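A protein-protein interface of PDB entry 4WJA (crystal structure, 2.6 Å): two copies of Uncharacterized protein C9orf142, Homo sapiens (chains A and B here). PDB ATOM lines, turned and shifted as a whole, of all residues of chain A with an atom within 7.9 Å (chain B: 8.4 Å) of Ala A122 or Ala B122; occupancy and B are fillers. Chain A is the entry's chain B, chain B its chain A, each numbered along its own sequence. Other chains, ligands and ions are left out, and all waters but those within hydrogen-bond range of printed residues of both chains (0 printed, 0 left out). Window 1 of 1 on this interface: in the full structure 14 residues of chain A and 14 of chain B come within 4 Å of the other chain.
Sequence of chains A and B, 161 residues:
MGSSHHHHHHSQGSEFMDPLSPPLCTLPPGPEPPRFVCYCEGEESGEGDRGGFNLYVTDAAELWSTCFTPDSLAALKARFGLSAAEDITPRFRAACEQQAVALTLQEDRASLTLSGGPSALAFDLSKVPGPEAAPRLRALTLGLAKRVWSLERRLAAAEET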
ATOM      1  N   LEU A  55      16.299  24.196 -11.057  1.00  0.00           N
ATOM      2  CA  LEU A  55      17.050  24.909 -10.021  1.00  0.00           C
ATOM      3  C   LEU A  55      17.201  26.349 -10.420  1.00  0.00           C
ATOM      4  O   LEU A  55      17.393  26.682 -11.603  1.00  0.00           O
ATOM      5  CB  LEU A  55      18.458  24.348  -9.892  1.00  0.00           C
ATOM      6  CG  LEU A  55      18.524  22.901  -9.498  1.00  0.00           C
ATOM      7  CD1 LEU A  55      19.960  22.431  -9.551  1.00  0.00           C
ATOM      8  CD2 LEU A  55      17.951  22.724  -8.107  1.00  0.00           C
ATOM      9  N   THR A  66      18.222  26.407 -14.534  1.00  0.00           N
ATOM     10  CA  THR A  66      18.583  25.258 -15.349  1.00  0.00           C
ATOM     11  C   THR A  66      17.875  25.286 -16.674  1.00  0.00           C
ATOM     12  O   THR A  66      18.397  24.763 -17.674  1.00  0.00           O
ATOM     13  CB  THR A  66      18.229  23.949 -14.644  1.00  0.00           C
ATOM     14  OG1 THR A  66      17.032  24.122 -13.866  1.00  0.00           O
ATOM     15  CG2 THR A  66      19.348  23.550 -13.704  1.00  0.00           C
ATOM     16  N   PHE A  68      15.255  23.706 -17.832  1.00  0.00           N
ATOM     17  CA  PHE A  68      15.276  22.350 -18.329  1.00  0.00           C
ATOM     18  C   PHE A  68      14.174  22.159 -19.362  1.00  0.00           C
ATOM     19  O   PHE A  68      13.128  22.766 -19.278  1.00  0.00           O
ATOM     20  CB  PHE A  68      15.045  21.339 -17.183  1.00  0.00           C
ATOM     21  CG  PHE A  68      16.281  20.991 -16.408  1.00  0.00           C
ATOM     22  CD1 PHE A  68      17.464  20.648 -17.059  1.00  0.00           C
ATOM     23  CD2 PHE A  68      16.252  20.964 -15.021  1.00  0.00           C
ATOM     24  CE1 PHE A  68      18.613  20.339 -16.355  1.00  0.00           C
ATOM     25  CE2 PHE A  68      17.391  20.641 -14.313  1.00  0.00           C
ATOM     26  CZ  PHE A  68      18.572  20.339 -14.984  1.00  0.00           C
ATOM     27  N   LEU A  76      20.432  14.766 -18.211  1.00  0.00           N
ATOM     28  CA  LEU A  76      21.229  15.030 -17.028  1.00  0.00           C
ATOM     29  C   LEU A  76      21.006  13.917 -15.991  1.00  0.00           C
ATOM     30  O   LEU A  76      21.945  13.427 -15.391  1.00  0.00           O
ATOM     31  CB  LEU A  76      20.876  16.405 -16.467  1.00  0.00           C
ATOM     32  CG  LEU A  76      21.644  16.797 -15.210  1.00  0.00           C
ATOM     33  CD1 LEU A  76      22.196  18.211 -15.281  1.00  0.00           C
ATOM     34  CD2 LEU A  76      20.734  16.626 -14.003  1.00  0.00           C
ATOM     35  N   ARG A  79      23.443  11.484 -17.387  1.00  0.00           N
ATOM     36  CA  ARG A  79      24.865  11.626 -17.038  1.00  0.00           C
ATOM     37  C   ARG A  79      25.194  11.165 -15.604  1.00  0.00           C
ATOM     38  O   ARG A  79      26.357  10.925 -15.291  1.00  0.00           O
ATOM     39  CB  ARG A  79      25.318  13.068 -17.227  1.00  0.00           C
ATOM     40  CG  ARG A  79      25.404  13.463 -18.681  1.00  0.00           C
ATOM     41  CD  ARG A  79      25.706  14.946 -18.843  1.00  0.00           C
ATOM     42  NE  ARG A  79      24.593  15.790 -18.403  1.00  0.00           N
ATOM     43  CZ  ARG A  79      24.200  16.918 -19.000  1.00  0.00           C
ATOM     44  NH1 ARG A  79      24.821  17.388 -20.095  1.00  0.00           N
ATOM     45  NH2 ARG A  79      23.167  17.580 -18.488  1.00  0.00           N
ATOM     46  N   PHE A  80      24.166  11.083 -14.746  1.00  0.00           N
ATOM     47  CA  PHE A  80      24.265  10.570 -13.377  1.00  0.00           C
ATOM     48  C   PHE A  80      23.180   9.508 -13.066  1.00  0.00           C
ATOM     49  O   PHE A  80      22.617   8.844 -13.956  1.00  0.00           O
ATOM     50  CB  PHE A  80      24.264  11.775 -12.407  1.00  0.00           C
ATOM     51  CG  PHE A  80      25.039  12.986 -12.950  1.00  0.00           C
ATOM     52  CD1 PHE A  80      26.431  13.031 -12.904  1.00  0.00           C
ATOM     53  CD2 PHE A  80      24.381  14.046 -13.572  1.00  0.00           C
ATOM     54  CE1 PHE A  80      27.135  14.111 -13.446  1.00  0.00           C
ATOM     55  CE2 PHE A  80      25.082  15.121 -14.112  1.00  0.00           C
ATOM     56  CZ  PHE A  80      26.459  15.152 -14.055  1.00  0.00           C
ATOM     57  N   ALA A 102      28.467  24.172  -4.379  1.00  0.00           N
ATOM     58  CA  ALA A 102      29.393  25.091  -5.008  1.00  0.00           C
ATOM     59  C   ALA A 102      28.722  25.795  -6.187  1.00  0.00           C
ATOM     60  O   ALA A 102      27.781  25.276  -6.750  1.00  0.00           O
ATOM     61  CB  ALA A 102      30.608  24.333  -5.498  1.00  0.00           C
ATOM     62  N   SER A 111      27.141  27.775 -13.226  1.00  0.00           N
ATOM     63  CA  SER A 111      27.072  26.345 -12.946  1.00  0.00           C
ATOM     64  C   SER A 111      26.917  26.111 -11.455  1.00  0.00           C
ATOM     65  O   SER A 111      27.388  26.879 -10.657  1.00  0.00           O
ATOM     66  CB  SER A 111      28.332  25.638 -13.452  1.00  0.00           C
ATOM     67  OG  SER A 111      29.310  25.619 -12.445  1.00  0.00           O
ATOM     68  N   LEU A 112      26.237  25.039 -11.090  1.00  0.00           N
ATOM     69  CA  LEU A 112      25.930  24.742  -9.713  1.00  0.00           C
ATOM     70  C   LEU A 112      26.284  23.256  -9.458  1.00  0.00           C
ATOM     71  O   LEU A 112      25.952  22.411 -10.275  1.00  0.00           O
ATOM     72  CB  LEU A 112      24.451  25.002  -9.461  1.00  0.00           C
ATOM     73  CG  LEU A 112      23.946  24.969  -8.009  1.00  0.00           C
ATOM     74  CD1 LEU A 112      24.416  26.222  -7.300  1.00  0.00           C
ATOM     75  CD2 LEU A 112      22.440  24.899  -7.950  1.00  0.00           C
ATOM     76  N   THR A 113      26.938  22.949  -8.327  1.00  0.00           N
ATOM     77  CA  THR A 113      27.399  21.597  -8.041  1.00  0.00           C
ATOM     78  C   THR A 113      26.891  21.123  -6.702  1.00  0.00           C
ATOM     79  O   THR A 113      27.114  21.761  -5.685  1.00  0.00           O
ATOM     80  CB  THR A 113      28.946  21.474  -8.065  1.00  0.00           C
ATOM     81  OG1 THR A 113      29.499  21.917  -9.332  1.00  0.00           O
ATOM     82  CG2 THR A 113      29.360  20.041  -7.849  1.00  0.00           C
ATOM     83  N   LEU A 114      26.204  19.990  -6.713  1.00  0.00           N
ATOM     84  CA  LEU A 114      25.706  19.364  -5.497  1.00  0.00           C
ATOM     85  C   LEU A 114      26.674  18.280  -5.101  1.00  0.00           C
ATOM     86  O   LEU A 114      26.940  17.367  -5.890  1.00  0.00           O
ATOM     87  CB  LEU A 114      24.323  18.757  -5.723  1.00  0.00           C
ATOM     88  CG  LEU A 114      23.089  19.684  -5.777  1.00  0.00           C
ATOM     89  CD1 LEU A 114      23.231  20.798  -6.798  1.00  0.00           C
ATOM     90  CD2 LEU A 114      21.808  18.887  -6.051  1.00  0.00           C
ATOM     91  N   SER A 115      27.206  18.389  -3.884  1.00  0.00           N
ATOM     92  CA  SER A 115      28.239  17.492  -3.391  1.00  0.00           C
ATOM     93  C   SER A 115      27.743  16.802  -2.175  1.00  0.00           C
ATOM     94  O   SER A 115      28.504  16.100  -1.531  1.00  0.00           O
ATOM     95  CB  SER A 115      29.471  18.266  -2.948  1.00  0.00           C
ATOM     96  OG  SER A 115      30.055  18.948  -4.033  1.00  0.00           O
ATOM     97  N   SER A 119      27.364  10.653  -5.595  1.00  0.00           N
ATOM     98  CA  SER A 119      28.023  11.121  -6.769  1.00  0.00           C
ATOM     99  C   SER A 119      27.831  12.624  -6.682  1.00  0.00           C
ATOM    100  O   SER A 119      26.958  13.085  -5.946  1.00  0.00           O
ATOM    101  CB  SER A 119      27.377  10.504  -8.005  1.00  0.00           C
ATOM    102  OG  SER A 119      27.714  11.227  -9.183  1.00  0.00           O
ATOM    103  N   ALA A 120      28.681  13.365  -7.378  1.00  0.00           N
ATOM    104  CA  ALA A 120      28.508  14.793  -7.572  1.00  0.00           C
ATOM    105  C   ALA A 120      27.758  15.169  -8.851  1.00  0.00           C
ATOM    106  O   ALA A 120      28.102  14.716  -9.941  1.00  0.00           O
ATOM    107  CB  ALA A 120      29.858  15.480  -7.604  1.00  0.00           C
ATOM    108  N   LEU A 121      26.798  16.079  -8.709  1.00  0.00           N
ATOM    109  CA  LEU A 121      26.017  16.574  -9.837  1.00  0.00           C
ATOM    110  C   LEU A 121      26.396  17.994 -10.211  1.00  0.00           C
ATOM    111  O   LEU A 121      26.584  18.822  -9.346  1.00  0.00           O
ATOM    112  CB  LEU A 121      24.550  16.524  -9.479  1.00  0.00           C
ATOM    113  CG  LEU A 121      24.111  15.178  -8.903  1.00  0.00           C
ATOM    114  CD1 LEU A 121      22.666  15.262  -8.448  1.00  0.00           C
ATOM    115  CD2 LEU A 121      24.308  14.088  -9.944  1.00  0.00           C
ATOM    116  N   ALA A 122      26.471  18.252 -11.513  1.00  0.00           N
ATOM    117  CA  ALA A 122      26.754  19.562 -12.048  1.00  0.00           C
ATOM    118  C   ALA A 122      25.600  20.007 -12.972  1.00  0.00           C
ATOM    119  O   ALA A 122      25.111  19.224 -13.792  1.00  0.00           O
ATOM    120  CB  ALA A 122      28.061  19.549 -12.813  1.00  0.00           C
ATOM    121  N   PHE A 123      25.186  21.267 -12.821  1.00  0.00           N
ATOM    122  CA  PHE A 123      24.021  21.816 -13.511  1.00  0.00           C
ATOM    123  C   PHE A 123      24.439  23.058 -14.263  1.00  0.00           C
ATOM    124  O   PHE A 123      25.041  23.962 -13.694  1.00  0.00           O
ATOM    125  CB  PHE A 123      22.968  22.201 -12.490  1.00  0.00           C
ATOM    126  CG  PHE A 123      22.296  21.042 -11.854  1.00  0.00           C
ATOM    127  CD1 PHE A 123      21.217  20.472 -12.447  1.00  0.00           C
ATOM    128  CD2 PHE A 123      22.759  20.505 -10.687  1.00  0.00           C
ATOM    129  CE1 PHE A 123      20.583  19.388 -11.889  1.00  0.00           C
ATOM    130  CE2 PHE A 123      22.129  19.416 -10.116  1.00  0.00           C
ATOM    131  CZ  PHE A 123      21.039  18.847 -10.728  1.00  0.00           C
ATOM    132  N   ASP A 124      24.101  23.139 -15.532  1.00  0.00           N
ATOM    133  CA  ASP A 124      24.312  24.382 -16.253  1.00  0.00           C
ATOM    134  C   ASP A 124      23.125  25.285 -16.011  1.00  0.00           C
ATOM    135  O   ASP A 124      21.989  24.836 -16.070  1.00  0.00           O
ATOM    136  CB  ASP A 124      24.488  24.111 -17.718  1.00  0.00           C
ATOM    137  CG  ASP A 124      25.586  23.138 -17.956  1.00  0.00           C
ATOM    138  OD1 ASP A 124      26.744  23.590 -18.058  1.00  0.00           O
ATOM    139  OD2 ASP A 124      25.304  21.913 -17.976  1.00  0.00           O
ATOM    140  N   LEU A 125      23.412  26.545 -15.709  1.00  0.00           N
ATOM    141  CA  LEU A 125      22.378  27.525 -15.518  1.00  0.00           C
ATOM    142  C   LEU A 125      22.613  28.682 -16.443  1.00  0.00           C
ATOM    143  O   LEU A 125      23.738  29.110 -16.601  1.00  0.00           O
ATOM    144  CB  LEU A 125      22.326  28.012 -14.074  1.00  0.00           C
ATOM    145  CG  LEU A 125      21.743  26.955 -13.146  1.00  0.00           C
ATOM    146  CD1 LEU A 125      22.851  26.123 -12.539  1.00  0.00           C
ATOM    147  CD2 LEU A 125      20.903  27.557 -12.044  1.00  0.00           C
ATOM    148  N   LEU B  55      42.846  13.445 -12.952  1.00  0.00           N
ATOM    149  CA  LEU B  55      42.946  14.725 -12.316  1.00  0.00           C
ATOM    150  C   LEU B  55      43.324  14.520 -10.851  1.00  0.00           C
ATOM    151  O   LEU B  55      42.881  13.578 -10.197  1.00  0.00           O
ATOM    152  CB  LEU B  55      41.607  15.421 -12.341  1.00  0.00           C
ATOM    153  CG  LEU B  55      41.047  15.715 -13.706  1.00  0.00           C
ATOM    154  CD1 LEU B  55      39.664  16.316 -13.546  1.00  0.00           C
ATOM    155  CD2 LEU B  55      41.952  16.690 -14.415  1.00  0.00           C
ATOM    156  N   THR B  66      40.970  11.348  -9.383  1.00  0.00           N
ATOM    157  CA  THR B  66      39.884  10.674 -10.082  1.00  0.00           C
ATOM    158  C   THR B  66      39.981   9.151  -9.971  1.00  0.00           C
ATOM    159  O   THR B  66      38.980   8.478 -10.032  1.00  0.00           O
ATOM    160  CB  THR B  66      39.853  11.057 -11.570  1.00  0.00           C
ATOM    161  OG1 THR B  66      41.193  11.218 -12.042  1.00  0.00           O
ATOM    162  CG2 THR B  66      39.078  12.382 -11.747  1.00  0.00           C
ATOM    163  N   PHE B  68      41.129   6.844 -12.198  1.00  0.00           N
ATOM    164  CA  PHE B  68      40.522   6.254 -13.384  1.00  0.00           C
ATOM    165  C   PHE B  68      41.124   4.921 -13.712  1.00  0.00           C
ATOM    166  O   PHE B  68      42.275   4.696 -13.452  1.00  0.00           O
ATOM    167  CB  PHE B  68      40.699   7.178 -14.626  1.00  0.00           C
ATOM    168  CG  PHE B  68      39.754   8.331 -14.661  1.00  0.00           C
ATOM    169  CD1 PHE B  68      38.399   8.128 -14.414  1.00  0.00           C
ATOM    170  CD2 PHE B  68      40.202   9.626 -14.935  1.00  0.00           C
ATOM    171  CE1 PHE B  68      37.514   9.197 -14.414  1.00  0.00           C
ATOM    172  CE2 PHE B  68      39.315  10.704 -14.926  1.00  0.00           C
ATOM    173  CZ  PHE B  68      37.960  10.487 -14.677  1.00  0.00           C
ATOM    174  N   LEU B  76      33.195   7.612 -18.642  1.00  0.00           N
ATOM    175  CA  LEU B  76      32.908   8.986 -18.263  1.00  0.00           C
ATOM    176  C   LEU B  76      32.919   9.844 -19.523  1.00  0.00           C
ATOM    177  O   LEU B  76      32.080  10.713 -19.698  1.00  0.00           O
ATOM    178  CB  LEU B  76      33.907   9.483 -17.207  1.00  0.00           C
ATOM    179  CG  LEU B  76      33.735  10.940 -16.749  1.00  0.00           C
ATOM    180  CD1 LEU B  76      33.813  11.108 -15.245  1.00  0.00           C
ATOM    181  CD2 LEU B  76      34.766  11.817 -17.437  1.00  0.00           C
ATOM    182  N   ARG B  79      29.441   9.151 -20.578  1.00  0.00           N
ATOM    183  CA  ARG B  79      28.324   9.819 -19.901  1.00  0.00           C
ATOM    184  C   ARG B  79      28.072  11.244 -20.337  1.00  0.00           C
ATOM    185  O   ARG B  79      26.958  11.745 -20.216  1.00  0.00           O
ATOM    186  CB  ARG B  79      28.556   9.828 -18.396  1.00  0.00           C
ATOM    187  CG  ARG B  79      28.533   8.461 -17.751  1.00  0.00           C
ATOM    188  CD  ARG B  79      29.403   8.422 -16.524  1.00  0.00           C
ATOM    189  NE  ARG B  79      28.744   9.133 -15.434  1.00  0.00           N
ATOM    190  CZ  ARG B  79      29.353   9.912 -14.537  1.00  0.00           C
ATOM    191  NH1 ARG B  79      30.673  10.112 -14.579  1.00  0.00           N
ATOM    192  NH2 ARG B  79      28.618  10.506 -13.592  1.00  0.00           N
ATOM    193  N   PHE B  80      29.129  11.909 -20.779  1.00  0.00           N
ATOM    194  CA  PHE B  80      29.019  13.161 -21.513  1.00  0.00           C
ATOM    195  C   PHE B  80      30.189  13.077 -22.476  1.00  0.00           C
ATOM    196  O   PHE B  80      30.797  12.025 -22.565  1.00  0.00           O
ATOM    197  CB  PHE B  80      29.081  14.432 -20.602  1.00  0.00           C
ATOM    198  CG  PHE B  80      29.743  14.247 -19.232  1.00  0.00           C
ATOM    199  CD1 PHE B  80      31.030  13.722 -19.091  1.00  0.00           C
ATOM    200  CD2 PHE B  80      29.100  14.724 -18.080  1.00  0.00           C
ATOM    201  CE1 PHE B  80      31.606  13.621 -17.832  1.00  0.00           C
ATOM    202  CE2 PHE B  80      29.676  14.618 -16.826  1.00  0.00           C
ATOM    203  CZ  PHE B  80      30.928  14.071 -16.702  1.00  0.00           C
ATOM    204  N   ALA B 102      35.647  24.860  -9.774  1.00  0.00           N
ATOM    205  CA  ALA B 102      35.099  24.776  -8.428  1.00  0.00           C
ATOM    206  C   ALA B 102      35.540  23.469  -7.808  1.00  0.00           C
ATOM    207  O   ALA B 102      35.845  22.506  -8.510  1.00  0.00           O
ATOM    208  CB  ALA B 102      33.585  24.835  -8.465  1.00  0.00           C
ATOM    209  N   ALA B 110      35.843  14.123  -2.595  1.00  0.00           N
ATOM    210  CA  ALA B 110      35.957  15.444  -3.144  1.00  0.00           C
ATOM    211  C   ALA B 110      35.288  15.467  -4.486  1.00  0.00           C
ATOM    212  O   ALA B 110      34.935  14.424  -5.023  1.00  0.00           O
ATOM    213  CB  ALA B 110      37.414  15.787  -3.310  1.00  0.00           C
ATOM    214  N   SER B 111      35.130  16.661  -5.034  1.00  0.00           N
ATOM    215  CA  SER B 111      34.586  16.800  -6.372  1.00  0.00           C
ATOM    216  C   SER B 111      35.189  18.026  -6.996  1.00  0.00           C
ATOM    217  O   SER B 111      35.471  18.995  -6.314  1.00  0.00           O
ATOM    218  CB  SER B 111      33.070  16.951  -6.343  1.00  0.00           C
ATOM    219  OG  SER B 111      32.717  18.339  -6.277  1.00  0.00           O
ATOM    220  N   LEU B 112      35.350  17.980  -8.299  1.00  0.00           N
ATOM    221  CA  LEU B 112      35.960  19.033  -9.024  1.00  0.00           C
ATOM    222  C   LEU B 112      35.095  19.324 -10.261  1.00  0.00           C
ATOM    223  O   LEU B 112      34.678  18.410 -10.978  1.00  0.00           O
ATOM    224  CB  LEU B 112      37.349  18.565  -9.459  1.00  0.00           C
ATOM    225  CG  LEU B 112      38.283  19.625 -10.031  1.00  0.00           C
ATOM    226  CD1 LEU B 112      38.762  20.529  -8.916  1.00  0.00           C
ATOM    227  CD2 LEU B 112      39.451  18.975 -10.726  1.00  0.00           C
ATOM    228  N   THR B 113      34.819  20.594 -10.501  1.00  0.00           N
ATOM    229  CA  THR B 113      33.903  20.968 -11.559  1.00  0.00           C
ATOM    230  C   THR B 113      34.591  21.896 -12.537  1.00  0.00           C
ATOM    231  O   THR B 113      35.104  22.936 -12.142  1.00  0.00           O
ATOM    232  CB  THR B 113      32.631  21.652 -10.997  1.00  0.00           C
ATOM    233  OG1 THR B 113      31.982  20.795 -10.028  1.00  0.00           O
ATOM    234  CG2 THR B 113      31.670  21.975 -12.144  1.00  0.00           C
ATOM    235  N   LEU B 114      34.566  21.520 -13.808  1.00  0.00           N
ATOM    236  CA  LEU B 114      35.090  22.341 -14.882  1.00  0.00           C
ATOM    237  C   LEU B 114      33.938  23.084 -15.550  1.00  0.00           C
ATOM    238  O   LEU B 114      33.006  22.462 -16.067  1.00  0.00           O
ATOM    239  CB  LEU B 114      35.800  21.473 -15.924  1.00  0.00           C
ATOM    240  CG  LEU B 114      37.205  20.935 -15.586  1.00  0.00           C
ATOM    241  CD1 LEU B 114      37.260  20.151 -14.288  1.00  0.00           C
ATOM    242  CD2 LEU B 114      37.733  20.079 -16.726  1.00  0.00           C
ATOM    243  N   SER B 115      34.018  24.415 -15.541  1.00  0.00           N
ATOM    244  CA  SER B 115      32.973  25.289 -16.097  1.00  0.00           C
ATOM    245  C   SER B 115      33.423  26.035 -17.346  1.00  0.00           C
ATOM    246  O   SER B 115      33.004  27.157 -17.573  1.00  0.00           O
ATOM    247  CB  SER B 115      32.502  26.286 -15.027  1.00  0.00           C
ATOM    248  OG  SER B 115      31.955  25.615 -13.907  1.00  0.00           O
ATOM    249  N   SER B 119      29.080  21.830 -21.863  1.00  0.00           N
ATOM    250  CA  SER B 119      28.404  21.537 -20.619  1.00  0.00           C
ATOM    251  C   SER B 119      29.418  21.409 -19.482  1.00  0.00           C
ATOM    252  O   SER B 119      30.571  21.051 -19.688  1.00  0.00           O
ATOM    253  CB  SER B 119      27.588  20.257 -20.817  1.00  0.00           C
ATOM    254  OG  SER B 119      27.036  19.773 -19.606  1.00  0.00           O
ATOM    255  N   ALA B 120      28.980  21.721 -18.273  1.00  0.00           N
ATOM    256  CA  ALA B 120      29.838  21.642 -17.112  1.00  0.00           C
ATOM    257  C   ALA B 120      30.126  20.195 -16.808  1.00  0.00           C
ATOM    258  O   ALA B 120      29.211  19.395 -16.771  1.00  0.00           O
ATOM    259  CB  ALA B 120      29.161  22.266 -15.916  1.00  0.00           C
ATOM    260  N   LEU B 121      31.397  19.893 -16.540  1.00  0.00           N
ATOM    261  CA  LEU B 121      31.832  18.546 -16.182  1.00  0.00           C
ATOM    262  C   LEU B 121      32.147  18.428 -14.697  1.00  0.00           C
ATOM    263  O   LEU B 121      32.726  19.307 -14.106  1.00  0.00           O
ATOM    264  CB  LEU B 121      33.059  18.182 -16.990  1.00  0.00           C
ATOM    265  CG  LEU B 121      32.837  18.425 -18.470  1.00  0.00           C
ATOM    266  CD1 LEU B 121      34.126  18.122 -19.195  1.00  0.00           C
ATOM    267  CD2 LEU B 121      31.690  17.578 -19.011  1.00  0.00           C
ATOM    268  N   ALA B 122      31.742  17.326 -14.104  1.00  0.00           N
ATOM    269  CA  ALA B 122      31.974  17.071 -12.694  1.00  0.00           C
ATOM    270  C   ALA B 122      32.765  15.778 -12.553  1.00  0.00           C
ATOM    271  O   ALA B 122      32.515  14.821 -13.284  1.00  0.00           O
ATOM    272  CB  ALA B 122      30.645  16.960 -11.961  1.00  0.00           C
ATOM    273  N   PHE B 123      33.708  15.764 -11.610  1.00  0.00           N
ATOM    274  CA  PHE B 123      34.599  14.633 -11.382  1.00  0.00           C
ATOM    275  C   PHE B 123      34.607  14.236  -9.940  1.00  0.00           C
ATOM    276  O   PHE B 123      34.758  15.070  -9.073  1.00  0.00           O
ATOM    277  CB  PHE B 123      35.976  15.046 -11.771  1.00  0.00           C
ATOM    278  CG  PHE B 123      36.139  15.192 -13.228  1.00  0.00           C
ATOM    279  CD1 PHE B 123      36.410  14.080 -14.026  1.00  0.00           C
ATOM    280  CD2 PHE B 123      35.984  16.414 -13.820  1.00  0.00           C
ATOM    281  CE1 PHE B 123      36.574  14.208 -15.400  1.00  0.00           C
ATOM    282  CE2 PHE B 123      36.157  16.558 -15.200  1.00  0.00           C
ATOM    283  CZ  PHE B 123      36.452  15.457 -15.987  1.00  0.00           C
ATOM    284  N   ASP B 124      34.338  12.978  -9.670  1.00  0.00           N
ATOM    285  CA  ASP B 124      34.441  12.491  -8.327  1.00  0.00           C
ATOM    286  C   ASP B 124      35.870  12.138  -8.092  1.00  0.00           C
ATOM    287  O   ASP B 124      36.528  11.496  -8.940  1.00  0.00           O
ATOM    288  CB  ASP B 124      33.551  11.283  -8.107  1.00  0.00           C
ATOM    289  CG  ASP B 124      32.104  11.569  -8.431  1.00  0.00           C
ATOM    290  OD1 ASP B 124      31.401  12.131  -7.556  1.00  0.00           O
ATOM    291  OD2 ASP B 124      31.696  11.263  -9.562  1.00  0.00           O
ATOM    292  N   LEU B 125      36.380  12.627  -6.975  1.00  0.00           N
ATOM    293  CA  LEU B 125      37.759  12.353  -6.574  1.00  0.00           C
ATOM    294  C   LEU B 125      37.737  11.716  -5.231  1.00  0.00           C
ATOM    295  O   LEU B 125      36.938  12.090  -4.390  1.00  0.00           O
ATOM    296  CB  LEU B 125      38.579  13.626  -6.526  1.00  0.00           C
ATOM    297  CG  LEU B 125      38.923  14.154  -7.920  1.00  0.00           C
ATOM    298  CD1 LEU B 125      37.898  15.154  -8.376  1.00  0.00           C
ATOM    299  CD2 LEU B 125      40.300  14.803  -7.962  1.00  0.00           C
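Arg A79 touches Phe B80, and with the chains exchanged Phe A80 touches Arg B79.
Ser A119 touches Asp B124, and with the chains exchanged Asp A124 touches Ser B119.
Ala A120 touches Ser B111, but with the chains exchanged Ser A111 does not touch Ala B120 (4.3 Å).
Ala A120 touches Asp B124, and with the chains exchanged Asp A124 touches Ala B120.
Positions printed for both chains: 55, 66, 68, 76, 79, 80, 102, 111, 112, 113, 114, 115, 119, 120, 121, 122, 123, 124 and 125.
NH1 of Arg A79 sits at hydrogen-bond distance from OG of Ser B119.
The side-chain hydroxyl (OG) of Ser B119 sits at hydrogen-bond distance from the side-chain carboxylate (OD2) of Asp A124, 3.2 Å away.
OG of Ser B115 lies within hydrogen-bond range of OG of Ser A111, at 3.0 Å.
NH2 of Arg B79 sits at hydrogen-bond distance from O of Arg A79, at 2.9 Å.
OD1 of Asp B124 lies within hydrogen-bond range of N of Ala A120 (3.0 Å).
OG1 of Thr A113 sits at hydrogen-bond distance from OG1 of Thr B113.
N of Ala B120 is in hydrogen-bond range of OD1 of Asp A124, at 2.9 Å.
The backbone NH of Thr A113 is in hydrogen-bond range of the backbone carbonyl oxygen of Ala A102 (2.9 Å).
N of Thr B113 sits at hydrogen-bond distance from O of Ala B102, 2.9 Å away.
Ala A122 touches just one residue of chain B: Ala B122.
Ala B122 touches just these residues of chain A: Ala A120 and Ala A122.
Printed residues of chain B within 4 Å of Ser A111: Ser B115 (3.0 Å).
Printed residues of chain A within 4 Å of Ser B119: Arg A79 and Asp A124.
Of the printed residues of chain B, Ser A119 touches Asp B124.
Printed residues of chain A within 4 Å of Ala B120: Asp A124.
Printed residues of chain A within 4 Å of Ser B115: Ser A111 (3.0 Å).
Ala A102 touches none of the printed residues of chain B.
Leu A121 touches none of the printed residues of chain B.
Hydrophobic or aromatic side chains of chain A that line the printed part of chain B: Phe A80, Ala A120 and Ala A122.
Hydrophobic or aromatic side chains of chain B that line the printed part of chain A: Phe B80, Ala B120 and Ala B122.
Arg A79 touches Phe B80.
NH2 of Arg B79 touches CD1 of Phe A80, at 3.4 Å.
Ser B111 touches Ser A115 (OG to OG, 3.5 Å).
Asp B124 touches Ser A119 (OD1 to CA, 3.6 Å).
Ser B111 touches Ala A120.
Ala A120 touches Ala B122.
Ala A122 touches Ala B122.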
